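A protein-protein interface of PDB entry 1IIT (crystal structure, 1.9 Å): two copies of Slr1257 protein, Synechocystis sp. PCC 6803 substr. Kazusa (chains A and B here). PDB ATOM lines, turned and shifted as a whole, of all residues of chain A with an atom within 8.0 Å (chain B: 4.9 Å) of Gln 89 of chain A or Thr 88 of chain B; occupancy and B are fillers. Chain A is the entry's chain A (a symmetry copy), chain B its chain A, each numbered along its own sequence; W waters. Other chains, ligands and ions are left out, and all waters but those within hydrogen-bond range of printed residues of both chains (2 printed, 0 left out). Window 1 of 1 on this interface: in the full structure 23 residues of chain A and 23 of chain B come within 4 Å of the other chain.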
ATOM      1  N   VAL A  34      -6.332   3.258 -24.052  1.00  0.00           N
ATOM      2  CA  VAL A  34      -6.885   1.919 -23.829  1.00  0.00           C
ATOM      3  C   VAL A  34      -6.866   1.597 -22.340  1.00  0.00           C
ATOM      4  O   VAL A  34      -7.895   1.233 -21.765  1.00  0.00           O
ATOM      5  CB  VAL A  34      -6.089   0.834 -24.588  1.00  0.00           C
ATOM      6  CG1 VAL A  34      -6.525  -0.558 -24.137  1.00  0.00           C
ATOM      7  CG2 VAL A  34      -6.301   0.981 -26.089  1.00  0.00           C
ATOM      8  N   VAL A  75       3.356  -9.384 -28.795  1.00  0.00           N
ATOM      9  CA  VAL A  75       3.184 -10.683 -28.149  1.00  0.00           C
ATOM     10  C   VAL A  75       3.996 -11.663 -28.982  1.00  0.00           C
ATOM     11  O   VAL A  75       3.610 -12.004 -30.101  1.00  0.00           O
ATOM     12  CB  VAL A  75       1.713 -11.146 -28.152  1.00  0.00           C
ATOM     13  CG1 VAL A  75       1.558 -12.394 -27.288  1.00  0.00           C
ATOM     14  CG2 VAL A  75       0.791 -10.029 -27.657  1.00  0.00           C
ATOM     15  N   THR A  86       1.928 -13.224 -18.030  1.00  0.00           N
ATOM     16  CA  THR A  86       0.915 -13.637 -18.992  1.00  0.00           C
ATOM     17  C   THR A  86       0.471 -12.398 -19.772  1.00  0.00           C
ATOM     18  O   THR A  86       0.406 -11.304 -19.220  1.00  0.00           O
ATOM     19  CB  THR A  86      -0.327 -14.263 -18.289  1.00  0.00           C
ATOM     20  OG1 THR A  86      -1.234 -14.755 -19.284  1.00  0.00           O
ATOM     21  CG2 THR A  86      -1.065 -13.226 -17.429  1.00  0.00           C
ATOM     22  N   PHE A  87       0.208 -12.561 -21.062  1.00  0.00           N
ATOM     23  CA  PHE A  87      -0.246 -11.435 -21.876  1.00  0.00           C
ATOM     24  C   PHE A  87      -1.762 -11.340 -21.873  1.00  0.00           C
ATOM     25  O   PHE A  87      -2.446 -12.346 -21.711  1.00  0.00           O
ATOM     26  CB  PHE A  87       0.206 -11.604 -23.325  1.00  0.00           C
ATOM     27  CG  PHE A  87       1.588 -11.124 -23.589  1.00  0.00           C
ATOM     28  CD1 PHE A  87       2.665 -11.998 -23.529  1.00  0.00           C
ATOM     29  CD2 PHE A  87       1.814  -9.798 -23.941  1.00  0.00           C
ATOM     30  CE1 PHE A  87       3.946 -11.559 -23.823  1.00  0.00           C
ATOM     31  CE2 PHE A  87       3.086  -9.352 -24.238  1.00  0.00           C
ATOM     32  CZ  PHE A  87       4.156 -10.232 -24.179  1.00  0.00           C
ATOM     33  N   THR A  88      -2.287 -10.129 -22.029  1.00  0.00           N
ATOM     34  CA  THR A  88      -3.727  -9.955 -22.138  1.00  0.00           C
ATOM     35  C   THR A  88      -4.030 -10.303 -23.596  1.00  0.00           C
ATOM     36  O   THR A  88      -3.120 -10.565 -24.388  1.00  0.00           O
ATOM     37  CB  THR A  88      -4.166  -8.484 -22.001  1.00  0.00           C
ATOM     38  OG1 THR A  88      -3.546  -7.711 -23.040  1.00  0.00           O
ATOM     39  CG2 THR A  88      -3.844  -7.916 -20.625  1.00  0.00           C
ATOM     40  N   GLN A  89      -5.306 -10.280 -23.954  1.00  0.00           N
ATOM     41  CA  GLN A  89      -5.690 -10.507 -25.336  1.00  0.00           C
ATOM     42  C   GLN A  89      -5.120  -9.305 -26.089  1.00  0.00           C
ATOM     43  O   GLN A  89      -4.955  -8.221 -25.508  1.00  0.00           O
ATOM     44  CB  GLN A  89      -7.215 -10.529 -25.464  1.00  0.00           C
ATOM     45  CG  GLN A  89      -7.836 -11.878 -25.135  1.00  0.00           C
ATOM     46  CD  GLN A  89      -7.409 -12.948 -26.122  1.00  0.00           C
ATOM     47  OE1 GLN A  89      -7.441 -12.732 -27.332  1.00  0.00           O
ATOM     48  NE2 GLN A  89      -6.975 -14.093 -25.613  1.00  0.00           N
ATOM     49  N   PRO A  90      -4.713  -9.502 -27.353  1.00  0.00           N
ATOM     50  CA  PRO A  90      -4.155  -8.403 -28.152  1.00  0.00           C
ATOM     51  C   PRO A  90      -5.202  -7.320 -28.410  1.00  0.00           C
ATOM     52  O   PRO A  90      -6.387  -7.624 -28.572  1.00  0.00           O
ATOM     53  CB  PRO A  90      -3.766  -9.091 -29.454  1.00  0.00           C
ATOM     54  CG  PRO A  90      -3.500 -10.498 -29.033  1.00  0.00           C
ATOM     55  CD  PRO A  90      -4.607 -10.781 -28.072  1.00  0.00           C
ATOM     56  N   TYR A  91      -4.761  -6.065 -28.454  1.00  0.00           N
ATOM     57  CA  TYR A  91      -5.666  -4.952 -28.694  1.00  0.00           C
ATOM     58  C   TYR A  91      -5.370  -4.208 -30.004  1.00  0.00           C
ATOM     59  O   TYR A  91      -6.146  -3.351 -30.424  1.00  0.00           O
ATOM     60  CB  TYR A  91      -5.653  -3.982 -27.500  1.00  0.00           C
ATOM     61  CG  TYR A  91      -4.367  -3.211 -27.322  1.00  0.00           C
ATOM     62  CD1 TYR A  91      -4.208  -1.947 -27.894  1.00  0.00           C
ATOM     63  CD2 TYR A  91      -3.296  -3.751 -26.608  1.00  0.00           C
ATOM     64  CE1 TYR A  91      -3.013  -1.243 -27.770  1.00  0.00           C
ATOM     65  CE2 TYR A  91      -2.091  -3.054 -26.480  1.00  0.00           C
ATOM     66  CZ  TYR A  91      -1.961  -1.800 -27.067  1.00  0.00           C
ATOM     67  OH  TYR A  91      -0.777  -1.115 -26.976  1.00  0.00           O
ATOM     68  N   PHE A  92      -4.278  -4.570 -30.669  1.00  0.00           N
ATOM     69  CA  PHE A  92      -3.884  -3.911 -31.917  1.00  0.00           C
ATOM     70  C   PHE A  92      -3.026  -4.851 -32.745  1.00  0.00           C
ATOM     71  O   PHE A  92      -2.251  -5.634 -32.209  1.00  0.00           O
ATOM     72  CB  PHE A  92      -3.081  -2.628 -31.620  1.00  0.00           C
ATOM     73  CG  PHE A  92      -2.814  -1.767 -32.841  1.00  0.00           C
ATOM     74  CD1 PHE A  92      -3.765  -0.854 -33.289  1.00  0.00           C
ATOM     75  CD2 PHE A  92      -1.612  -1.871 -33.540  1.00  0.00           C
ATOM     76  CE1 PHE A  92      -3.524  -0.055 -34.425  1.00  0.00           C
ATOM     77  CE2 PHE A  92      -1.360  -1.082 -34.674  1.00  0.00           C
ATOM     78  CZ  PHE A  92      -2.320  -0.173 -35.115  1.00  0.00           C
ATOM     79  N   PRO A 189       0.830  -8.756 -32.982  1.00  0.00           N
ATOM     80  CA  PRO A 189      -0.239  -8.203 -32.152  1.00  0.00           C
ATOM     81  C   PRO A 189       0.359  -7.511 -30.916  1.00  0.00           C
ATOM     82  O   PRO A 189       1.450  -7.872 -30.464  1.00  0.00           O
ATOM     83  CB  PRO A 189      -1.045  -9.449 -31.780  1.00  0.00           C
ATOM     84  CG  PRO A 189      -0.016 -10.514 -31.695  1.00  0.00           C
ATOM     85  CD  PRO A 189       0.888 -10.226 -32.879  1.00  0.00           C
ATOM     86  N   TYR A 190      -0.313  -6.471 -30.427  1.00  0.00           N
ATOM     87  CA  TYR A 190       0.126  -5.751 -29.228  1.00  0.00           C
ATOM     88  C   TYR A 190      -0.779  -6.169 -28.073  1.00  0.00           C
ATOM     89  O   TYR A 190      -1.983  -6.280 -28.248  1.00  0.00           O
ATOM     90  CB  TYR A 190      -0.043  -4.233 -29.370  1.00  0.00           C
ATOM     91  CG  TYR A 190       0.894  -3.509 -30.305  1.00  0.00           C
ATOM     92  CD1 TYR A 190       0.608  -2.203 -30.695  1.00  0.00           C
ATOM     93  CD2 TYR A 190       2.065  -4.101 -30.786  1.00  0.00           C
ATOM     94  CE1 TYR A 190       1.449  -1.503 -31.536  1.00  0.00           C
ATOM     95  CE2 TYR A 190       2.924  -3.399 -31.639  1.00  0.00           C
ATOM     96  CZ  TYR A 190       2.601  -2.095 -32.007  1.00  0.00           C
ATOM     97  OH  TYR A 190       3.399  -1.377 -32.874  1.00  0.00           O
ATOM     98  N   GLY A 191      -0.191  -6.371 -26.898  1.00  0.00           N
ATOM     99  CA  GLY A 191      -0.958  -6.725 -25.715  1.00  0.00           C
ATOM    100  C   GLY A 191      -0.309  -6.094 -24.491  1.00  0.00           C
ATOM    101  O   GLY A 191       0.728  -5.429 -24.604  1.00  0.00           O
ATOM    102  N   PHE A 192      -0.952  -6.218 -23.335  1.00  0.00           N
ATOM    103  CA  PHE A 192      -0.391  -5.697 -22.091  1.00  0.00           C
ATOM    104  C   PHE A 192       0.137  -6.909 -21.315  1.00  0.00           C
ATOM    105  O   PHE A 192      -0.236  -8.046 -21.613  1.00  0.00           O
ATOM    106  CB  PHE A 192      -1.464  -4.980 -21.271  1.00  0.00           C
ATOM    107  CG  PHE A 192      -1.969  -3.697 -21.888  1.00  0.00           C
ATOM    108  CD1 PHE A 192      -3.181  -3.152 -21.467  1.00  0.00           C
ATOM    109  CD2 PHE A 192      -1.226  -3.013 -22.848  1.00  0.00           C
ATOM    110  CE1 PHE A 192      -3.645  -1.951 -21.978  1.00  0.00           C
ATOM    111  CE2 PHE A 192      -1.683  -1.802 -23.370  1.00  0.00           C
ATOM    112  CZ  PHE A 192      -2.895  -1.269 -22.934  1.00  0.00           C
ATOM    113  N   LEU A 194       0.594  -8.864 -17.620  1.00  0.00           N
ATOM    114  CA  LEU A 194       0.121  -9.015 -16.250  1.00  0.00           C
ATOM    115  C   LEU A 194       0.919 -10.134 -15.582  1.00  0.00           C
ATOM    116  O   LEU A 194       1.676 -10.851 -16.247  1.00  0.00           O
ATOM    117  CB  LEU A 194      -1.358  -9.415 -16.260  1.00  0.00           C
ATOM    118  CG  LEU A 194      -2.414  -8.390 -16.659  1.00  0.00           C
ATOM    119  CD1 LEU A 194      -3.733  -9.071 -17.003  1.00  0.00           C
ATOM    120  CD2 LEU A 194      -2.600  -7.432 -15.501  1.00  0.00           C
ATOM    121  N   GLN A 201      -6.739 -10.231 -14.512  1.00  0.00           N
ATOM    122  CA  GLN A 201      -6.759 -10.754 -15.881  1.00  0.00           C
ATOM    123  C   GLN A 201      -8.116 -10.799 -16.578  1.00  0.00           C
ATOM    124  O   GLN A 201      -8.305 -10.164 -17.619  1.00  0.00           O
ATOM    125  CB  GLN A 201      -6.096 -12.138 -15.924  1.00  0.00           C
ATOM    126  CG  GLN A 201      -5.937 -12.734 -17.315  1.00  0.00           C
ATOM    127  CD  GLN A 201      -5.132 -14.028 -17.301  1.00  0.00           C
ATOM    128  OE1 GLN A 201      -4.943 -14.645 -16.250  1.00  0.00           O
ATOM    129  NE2 GLN A 201      -4.644 -14.435 -18.467  1.00  0.00           N
ATOM    130  N   ILE A 204      -9.668  -7.299 -17.117  1.00  0.00           N
ATOM    131  CA  ILE A 204      -8.944  -6.535 -18.130  1.00  0.00           C
ATOM    132  C   ILE A 204      -9.233  -7.067 -19.536  1.00  0.00           C
ATOM    133  O   ILE A 204      -9.527  -6.286 -20.442  1.00  0.00           O
ATOM    134  CB  ILE A 204      -7.415  -6.488 -17.833  1.00  0.00           C
ATOM    135  CG1 ILE A 204      -7.172  -5.709 -16.527  1.00  0.00           C
ATOM    136  CG2 ILE A 204      -6.664  -5.825 -18.990  1.00  0.00           C
ATOM    137  CD1 ILE A 204      -5.704  -5.565 -16.127  1.00  0.00           C
ATOM    138  N   ASN A 205      -9.212  -8.388 -19.699  1.00  0.00           N
ATOM    139  CA  ASN A 205      -9.493  -8.993 -21.005  1.00  0.00           C
ATOM    140  C   ASN A 205     -10.885  -8.635 -21.519  1.00  0.00           C
ATOM    141  O   ASN A 205     -11.033  -8.200 -22.660  1.00  0.00           O
ATOM    142  CB  ASN A 205      -9.310 -10.517 -20.971  1.00  0.00           C
ATOM    143  CG  ASN A 205      -7.853 -10.930 -21.090  1.00  0.00           C
ATOM    144  OD1 ASN A 205      -7.043 -10.206 -21.666  1.00  0.00           O
ATOM    145  ND2 ASN A 205      -7.514 -12.098 -20.556  1.00  0.00           N
ATOM    146  N   VAL A 206     -11.895  -8.780 -20.664  1.00  0.00           N
ATOM    147  CA  VAL A 206     -13.274  -8.461 -21.041  1.00  0.00           C
ATOM    148  C   VAL A 206     -13.388  -7.003 -21.485  1.00  0.00           C
ATOM    149  O   VAL A 206     -13.950  -6.715 -22.543  1.00  0.00           O
ATOM    150  CB  VAL A 206     -14.261  -8.733 -19.869  1.00  0.00           C
ATOM    151  CG1 VAL A 206     -15.644  -8.166 -20.177  1.00  0.00           C
ATOM    152  CG2 VAL A 206     -14.341 -10.228 -19.595  1.00  0.00           C
ATOM    153  N   MET A 208     -10.946  -4.871 -22.470  1.00  0.00           N
ATOM    154  CA  MET A 208     -10.173  -4.594 -23.675  1.00  0.00           C
ATOM    155  C   MET A 208     -10.914  -5.142 -24.902  1.00  0.00           C
ATOM    156  O   MET A 208     -10.927  -4.517 -25.964  1.00  0.00           O
ATOM    157  CB  MET A 208      -8.777  -5.206 -23.566  1.00  0.00           C
ATOM    158  CG  MET A 208      -7.852  -4.434 -22.636  1.00  0.00           C
ATOM    159  SD  MET A 208      -6.289  -5.262 -22.395  1.00  0.00           S
ATOM    160  CE  MET A 208      -5.539  -5.036 -24.001  1.00  0.00           C
ATOM    161  N   LEU A 209     -11.567  -6.290 -24.735  1.00  0.00           N
ATOM    162  CA  LEU A 209     -12.324  -6.898 -25.823  1.00  0.00           C
ATOM    163  C   LEU A 209     -13.564  -6.046 -26.130  1.00  0.00           C
ATOM    164  O   LEU A 209     -13.939  -5.885 -27.293  1.00  0.00           O
ATOM    165  CB  LEU A 209     -12.686  -8.351 -25.482  1.00  0.00           C
ATOM    166  CG  LEU A 209     -11.516  -9.348 -25.562  1.00  0.00           C
ATOM    167  CD1 LEU A 209     -11.870 -10.664 -24.894  1.00  0.00           C
ATOM    168  CD2 LEU A 209     -11.129  -9.570 -27.023  1.00  0.00           C
ATOM    169  N   LEU A 212     -12.372  -3.103 -28.071  1.00  0.00           N
ATOM    170  CA  LEU A 212     -12.023  -3.571 -29.407  1.00  0.00           C
ATOM    171  C   LEU A 212     -13.267  -3.716 -30.285  1.00  0.00           C
ATOM    172  O   LEU A 212     -13.368  -3.077 -31.328  1.00  0.00           O
ATOM    173  CB  LEU A 212     -11.316  -4.921 -29.309  1.00  0.00           C
ATOM    174  CG  LEU A 212     -10.638  -5.441 -30.572  1.00  0.00           C
ATOM    175  CD1 LEU A 212      -9.481  -4.506 -30.942  1.00  0.00           C
ATOM    176  CD2 LEU A 212     -10.145  -6.865 -30.333  1.00  0.00           C
ATOM    177  N   ILE A 217     -11.219   1.389 -29.708  1.00  0.00           N
ATOM    178  CA  ILE A 217      -9.769   1.393 -29.880  1.00  0.00           C
ATOM    179  C   ILE A 217      -9.429   1.954 -31.263  1.00  0.00           C
ATOM    180  O   ILE A 217      -8.441   2.680 -31.417  1.00  0.00           O
ATOM    181  CB  ILE A 217      -9.155  -0.017 -29.677  1.00  0.00           C
ATOM    182  CG1 ILE A 217      -9.463  -0.515 -28.256  1.00  0.00           C
ATOM    183  CG2 ILE A 217      -7.648   0.028 -29.895  1.00  0.00           C
ATOM    184  CD1 ILE A 217      -8.836  -1.841 -27.904  1.00  0.00           C
ATOM    185  N   VAL B  75     -13.076 -15.003 -30.025  1.00  0.00           N
ATOM    186  CA  VAL B  75     -12.795 -14.456 -28.700  1.00  0.00           C
ATOM    187  C   VAL B  75     -13.647 -13.201 -28.587  1.00  0.00           C
ATOM    188  O   VAL B  75     -13.359 -12.189 -29.228  1.00  0.00           O
ATOM    189  CB  VAL B  75     -11.315 -14.054 -28.536  1.00  0.00           C
ATOM    190  CG1 VAL B  75     -11.032 -13.690 -27.082  1.00  0.00           C
ATOM    191  CG2 VAL B  75     -10.392 -15.183 -29.001  1.00  0.00           C
ATOM    192  N   THR B  86     -10.472 -19.234 -19.633  1.00  0.00           N
ATOM    193  CA  THR B  86      -9.542 -18.250 -20.170  1.00  0.00           C
ATOM    194  C   THR B  86      -9.222 -18.640 -21.614  1.00  0.00           C
ATOM    195  O   THR B  86      -9.145 -19.821 -21.938  1.00  0.00           O
ATOM    196  CB  THR B  86      -8.215 -18.204 -19.354  1.00  0.00           C
ATOM    197  OG1 THR B  86      -7.392 -17.142 -19.852  1.00  0.00           O
ATOM    198  CG2 THR B  86      -7.437 -19.522 -19.476  1.00  0.00           C
ATOM    199  N   PHE B  87      -9.079 -17.651 -22.487  1.00  0.00           N
ATOM    200  CA  PHE B  87      -8.749 -17.935 -23.883  1.00  0.00           C
ATOM    201  C   PHE B  87      -7.244 -17.952 -24.091  1.00  0.00           C
ATOM    202  O   PHE B  87      -6.510 -17.283 -23.368  1.00  0.00           O
ATOM    203  CB  PHE B  87      -9.332 -16.863 -24.801  1.00  0.00           C
ATOM    204  CG  PHE B  87     -10.750 -17.097 -25.181  1.00  0.00           C
ATOM    205  CD1 PHE B  87     -11.782 -16.524 -24.452  1.00  0.00           C
ATOM    206  CD2 PHE B  87     -11.058 -17.861 -26.301  1.00  0.00           C
ATOM    207  CE1 PHE B  87     -13.101 -16.704 -24.837  1.00  0.00           C
ATOM    208  CE2 PHE B  87     -12.368 -18.044 -26.695  1.00  0.00           C
ATOM    209  CZ  PHE B  87     -13.394 -17.466 -25.963  1.00  0.00           C
ATOM    210  N   THR B  88      -6.781 -18.732 -25.061  1.00  0.00           N
ATOM    211  CA  THR B  88      -5.366 -18.737 -25.397  1.00  0.00           C
ATOM    212  C   THR B  88      -5.193 -17.498 -26.276  1.00  0.00           C
ATOM    213  O   THR B  88      -6.165 -16.809 -26.601  1.00  0.00           O
ATOM    214  CB  THR B  88      -4.970 -19.910 -26.316  1.00  0.00           C
ATOM    215  OG1 THR B  88      -5.717 -19.820 -27.539  1.00  0.00           O
ATOM    216  CG2 THR B  88      -5.178 -21.260 -25.641  1.00  0.00           C
ATOM    217  N   GLN B  89      -3.960 -17.230 -26.680  1.00  0.00           N
ATOM    218  CA  GLN B  89      -3.703 -16.128 -27.590  1.00  0.00           C
ATOM    219  C   GLN B  89      -4.388 -16.546 -28.892  1.00  0.00           C
ATOM    220  O   GLN B  89      -4.535 -17.748 -29.166  1.00  0.00           O
ATOM    221  CB  GLN B  89      -2.198 -15.971 -27.819  1.00  0.00           C
ATOM    222  CG  GLN B  89      -1.498 -15.159 -26.739  1.00  0.00           C
ATOM    223  CD  GLN B  89      -1.979 -13.720 -26.719  1.00  0.00           C
ATOM    224  OE1 GLN B  89      -2.072 -13.077 -27.762  1.00  0.00           O
ATOM    225  NE2 GLN B  89      -2.319 -13.220 -25.539  1.00  0.00           N
ATOM    226  N   PRO B  90      -4.907 -15.575 -29.658  1.00  0.00           N
ATOM    227  CA  PRO B  90      -5.580 -15.885 -30.927  1.00  0.00           C
ATOM    228  C   PRO B  90      -4.604 -16.483 -31.939  1.00  0.00           C
ATOM    229  O   PRO B  90      -3.430 -16.105 -31.972  1.00  0.00           O
ATOM    230  CB  PRO B  90      -6.068 -14.521 -31.397  1.00  0.00           C
ATOM    231  CG  PRO B  90      -6.239 -13.760 -30.125  1.00  0.00           C
ATOM    232  CD  PRO B  90      -5.035 -14.146 -29.332  1.00  0.00           C
ATOM    233  N   GLY B 191      -9.476 -18.382 -30.964  1.00  0.00           N
ATOM    234  CA  GLY B 191      -8.586 -18.874 -29.926  1.00  0.00           C
ATOM    235  C   GLY B 191      -9.136 -20.182 -29.375  1.00  0.00           C
ATOM    236  O   GLY B 191     -10.203 -20.643 -29.800  1.00  0.00           O
ATOM    237  N   PHE B 192      -8.380 -20.834 -28.498  1.00  0.00           N
ATOM    238  CA  PHE B 192      -8.837 -22.071 -27.868  1.00  0.00           C
ATOM    239  C   PHE B 192      -9.242 -21.700 -26.436  1.00  0.00           C
ATOM    240  O   PHE B 192      -8.858 -20.640 -25.939  1.00  0.00           O
ATOM    241  CB  PHE B 192      -7.716 -23.111 -27.840  1.00  0.00           C
ATOM    242  CG  PHE B 192      -7.322 -23.641 -29.199  1.00  0.00           C
ATOM    243  CD1 PHE B 192      -6.095 -24.282 -29.367  1.00  0.00           C
ATOM    244  CD2 PHE B 192      -8.179 -23.541 -30.293  1.00  0.00           C
ATOM    245  CE1 PHE B 192      -5.728 -24.822 -30.588  1.00  0.00           C
ATOM    246  CE2 PHE B 192      -7.820 -24.081 -31.528  1.00  0.00           C
ATOM    247  CZ  PHE B 192      -6.592 -24.723 -31.677  1.00  0.00           C
ATOM    248  N   LEU B 194      -9.266 -22.712 -22.355  1.00  0.00           N
ATOM    249  CA  LEU B 194      -8.658 -23.493 -21.285  1.00  0.00           C
ATOM    250  C   LEU B 194      -9.346 -23.131 -19.969  1.00  0.00           C
ATOM    251  O   LEU B 194     -10.136 -22.181 -19.912  1.00  0.00           O
ATOM    252  CB  LEU B 194      -7.173 -23.132 -21.170  1.00  0.00           C
ATOM    253  CG  LEU B 194      -6.199 -23.594 -22.249  1.00  0.00           C
ATOM    254  CD1 LEU B 194      -4.896 -22.807 -22.179  1.00  0.00           C
ATOM    255  CD2 LEU B 194      -5.938 -25.072 -22.045  1.00  0.00           C
ATOM    256  N   ILE B 204       0.931 -23.836 -24.015  1.00  0.00           N
ATOM    257  CA  ILE B 204       0.084 -23.760 -25.204  1.00  0.00           C
ATOM    258  C   ILE B 204       0.255 -22.419 -25.920  1.00  0.00           C
ATOM    259  O   ILE B 204       0.431 -22.388 -27.139  1.00  0.00           O
ATOM    260  CB  ILE B 204      -1.409 -24.049 -24.867  1.00  0.00           C
ATOM    261  CG1 ILE B 204      -1.553 -25.507 -24.392  1.00  0.00           C
ATOM    262  CG2 ILE B 204      -2.292 -23.803 -26.092  1.00  0.00           C
ATOM    263  CD1 ILE B 204      -2.980 -25.934 -24.049  1.00  0.00           C
ATOM    264  N   ASN B 205       0.268 -21.324 -25.162  1.00  0.00           N
ATOM    265  CA  ASN B 205       0.443 -19.994 -25.755  1.00  0.00           C
ATOM    266  C   ASN B 205       1.764 -19.869 -26.508  1.00  0.00           C
ATOM    267  O   ASN B 205       1.786 -19.431 -27.658  1.00  0.00           O
ATOM    268  CB  ASN B 205       0.320 -18.886 -24.699  1.00  0.00           C
ATOM    269  CG  ASN B 205      -1.125 -18.553 -24.373  1.00  0.00           C
ATOM    270  OD1 ASN B 205      -2.013 -18.741 -25.202  1.00  0.00           O
ATOM    271  ND2 ASN B 205      -1.367 -18.048 -23.168  1.00  0.00           N
ATOM    272  N   MET B 208       1.594 -22.045 -29.719  1.00  0.00           N
ATOM    273  CA  MET B 208       0.699 -21.481 -30.722  1.00  0.00           C
ATOM    274  C   MET B 208       1.337 -20.229 -31.339  1.00  0.00           C
ATOM    275  O   MET B 208       1.224 -19.990 -32.542  1.00  0.00           O
ATOM    276  CB  MET B 208      -0.657 -21.147 -30.099  1.00  0.00           C
ATOM    277  CG  MET B 208      -1.515 -22.376 -29.833  1.00  0.00           C
ATOM    278  SD  MET B 208      -3.016 -21.976 -28.953  1.00  0.00           S
ATOM    279  CE  MET B 208      -3.926 -21.105 -30.221  1.00  0.00           C
HETATM  280  O   HOH W   1      -6.973 -14.568 -22.657  1.00  0.00           O
HETATM  281  O   HOH W   2      -2.017 -14.828 -23.032  1.00  0.00           O
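The side-chain hydroxyl (OG1) of Thr 88 of chain B lies close to the side-chain sulfur (SD) of Met 208 of chain B.
The side-chain amide oxygen of Asn 205 of chain B is in hydrogen-bond range of the backbone NH of Gln 89 of chain B, at 2.9 Å.
N of Val 75 of chain A sits at hydrogen-bond distance from O of Pro 189 of chain A (3.0 Å).
The backbone carbonyl oxygen (O) of Phe 192 of chain A is in hydrogen-bond range of the backbone NH (N) of Thr 88 of chain A (3.0 Å).
OG1 of Thr 88 of chain A lies close to SD of Met 208 of chain A (3.7 Å).
N of Gln 89 of chain A lies within hydrogen-bond range of OD1 of Asn 205 of chain A, at 2.9 Å.
The backbone carbonyl oxygen of Thr 88 of chain B lies within hydrogen-bond range of the side-chain amide nitrogen of Gln 89 of chain A, at 3.0 Å.
The side-chain amide nitrogen (NE2) of Gln 89 of chain B sits at hydrogen-bond distance from the backbone carbonyl oxygen (O) of Thr 88 of chain A, at 3.0 Å.
Val 75 of chain A touches Gln 89 of chain B, and with the chains exchanged Gln 89 of chain A touches Val 75 of chain B.
Phe 87 of chain A touches Gln 89 of chain B, and with the chains exchanged Gln 89 of chain A touches Phe 87 of chain B.
Thr 88 of chain A touches Gln 89 of chain B, and with the chains exchanged Gln 89 of chain A touches Thr 88 of chain B.
Pro 90 of chain B touches its own counterpart, Pro 90 of chain A.
Of the 10 pairs that touch across the chains among the printed residues, 9 have their exchanged pair printed and touching as well.
Of the 22 printed residues of chain A, 6 touch a printed residue of chain B.
Hydrophobic or aromatic side chains of chain A within 4 Å of the printed part of chain B: Val 75, Phe 87, Pro 90 and Leu 209.
Along chain A the printed residues that touch a printed residue of chain B span positions 75 to 209.
Printed residues of chain B that touch a printed residue of chain A: Val 75, Phe 87, Thr 88, Gln 89 and Pro 90.
Hydrophobic or aromatic side chains of chain B that line the printed part of chain A: Val 75, Phe 87 and Pro 90.
Among the printed residues, 10 pairs touch across the chains.
Water W1 lies within hydrogen-bond range of the backbone carbonyl oxygen of Phe 87 of chain B (2.8 Å), the side-chain amide nitrogen of Gln 89 of chain A (3.0 Å) and the side-chain amide nitrogen of Asn 205 of chain A (3.3 Å).
Water W2 lies within hydrogen-bond range of O of Phe 87 of chain A, NE2 of Gln 89 of chain B and ND2 of Asn 205 of chain B.
Val 75 of chain A touches Gln 89 of chain B (CG1 to OE1, 3.7 Å).
Gln 89 of chain B touches Phe 87 of chain A (NE2 to CB, 3.7 Å).
CG1 of Val 75 of chain B touches OE1 of Gln 89 of chain A (3.7 Å).
Gln 89 of chain A touches Phe 87 of chain B.
OE1 of Gln 89 of chain A touches CG of Pro 90 of chain B, at 3.2 Å.
Pro 90 of chain A touches Gln 89 of chain B (CG to OE1, 3.2 Å).
Pro 90 of chain A touches Pro 90 of chain B (CD to CD, 3.6 Å).
Val 75 of chain B touches Leu 209 of chain A.
Gln 89 of chain A touches just these residues of chain B: Val 75 (3.7 Å), Phe 87 (3.7 Å), Thr 88 (3.0 Å) and Pro 90 (3.2 Å).
Printed residues of chain B within 4 Å of Leu 209 of chain A: Val 75.
Printed residues of chain A within 4 Å of Pro 90 of chain B: Gln 89 (3.2 Å) and Pro 90 (3.6 Å).
Phe 192 of chain B touches none of the printed residues of chain A.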
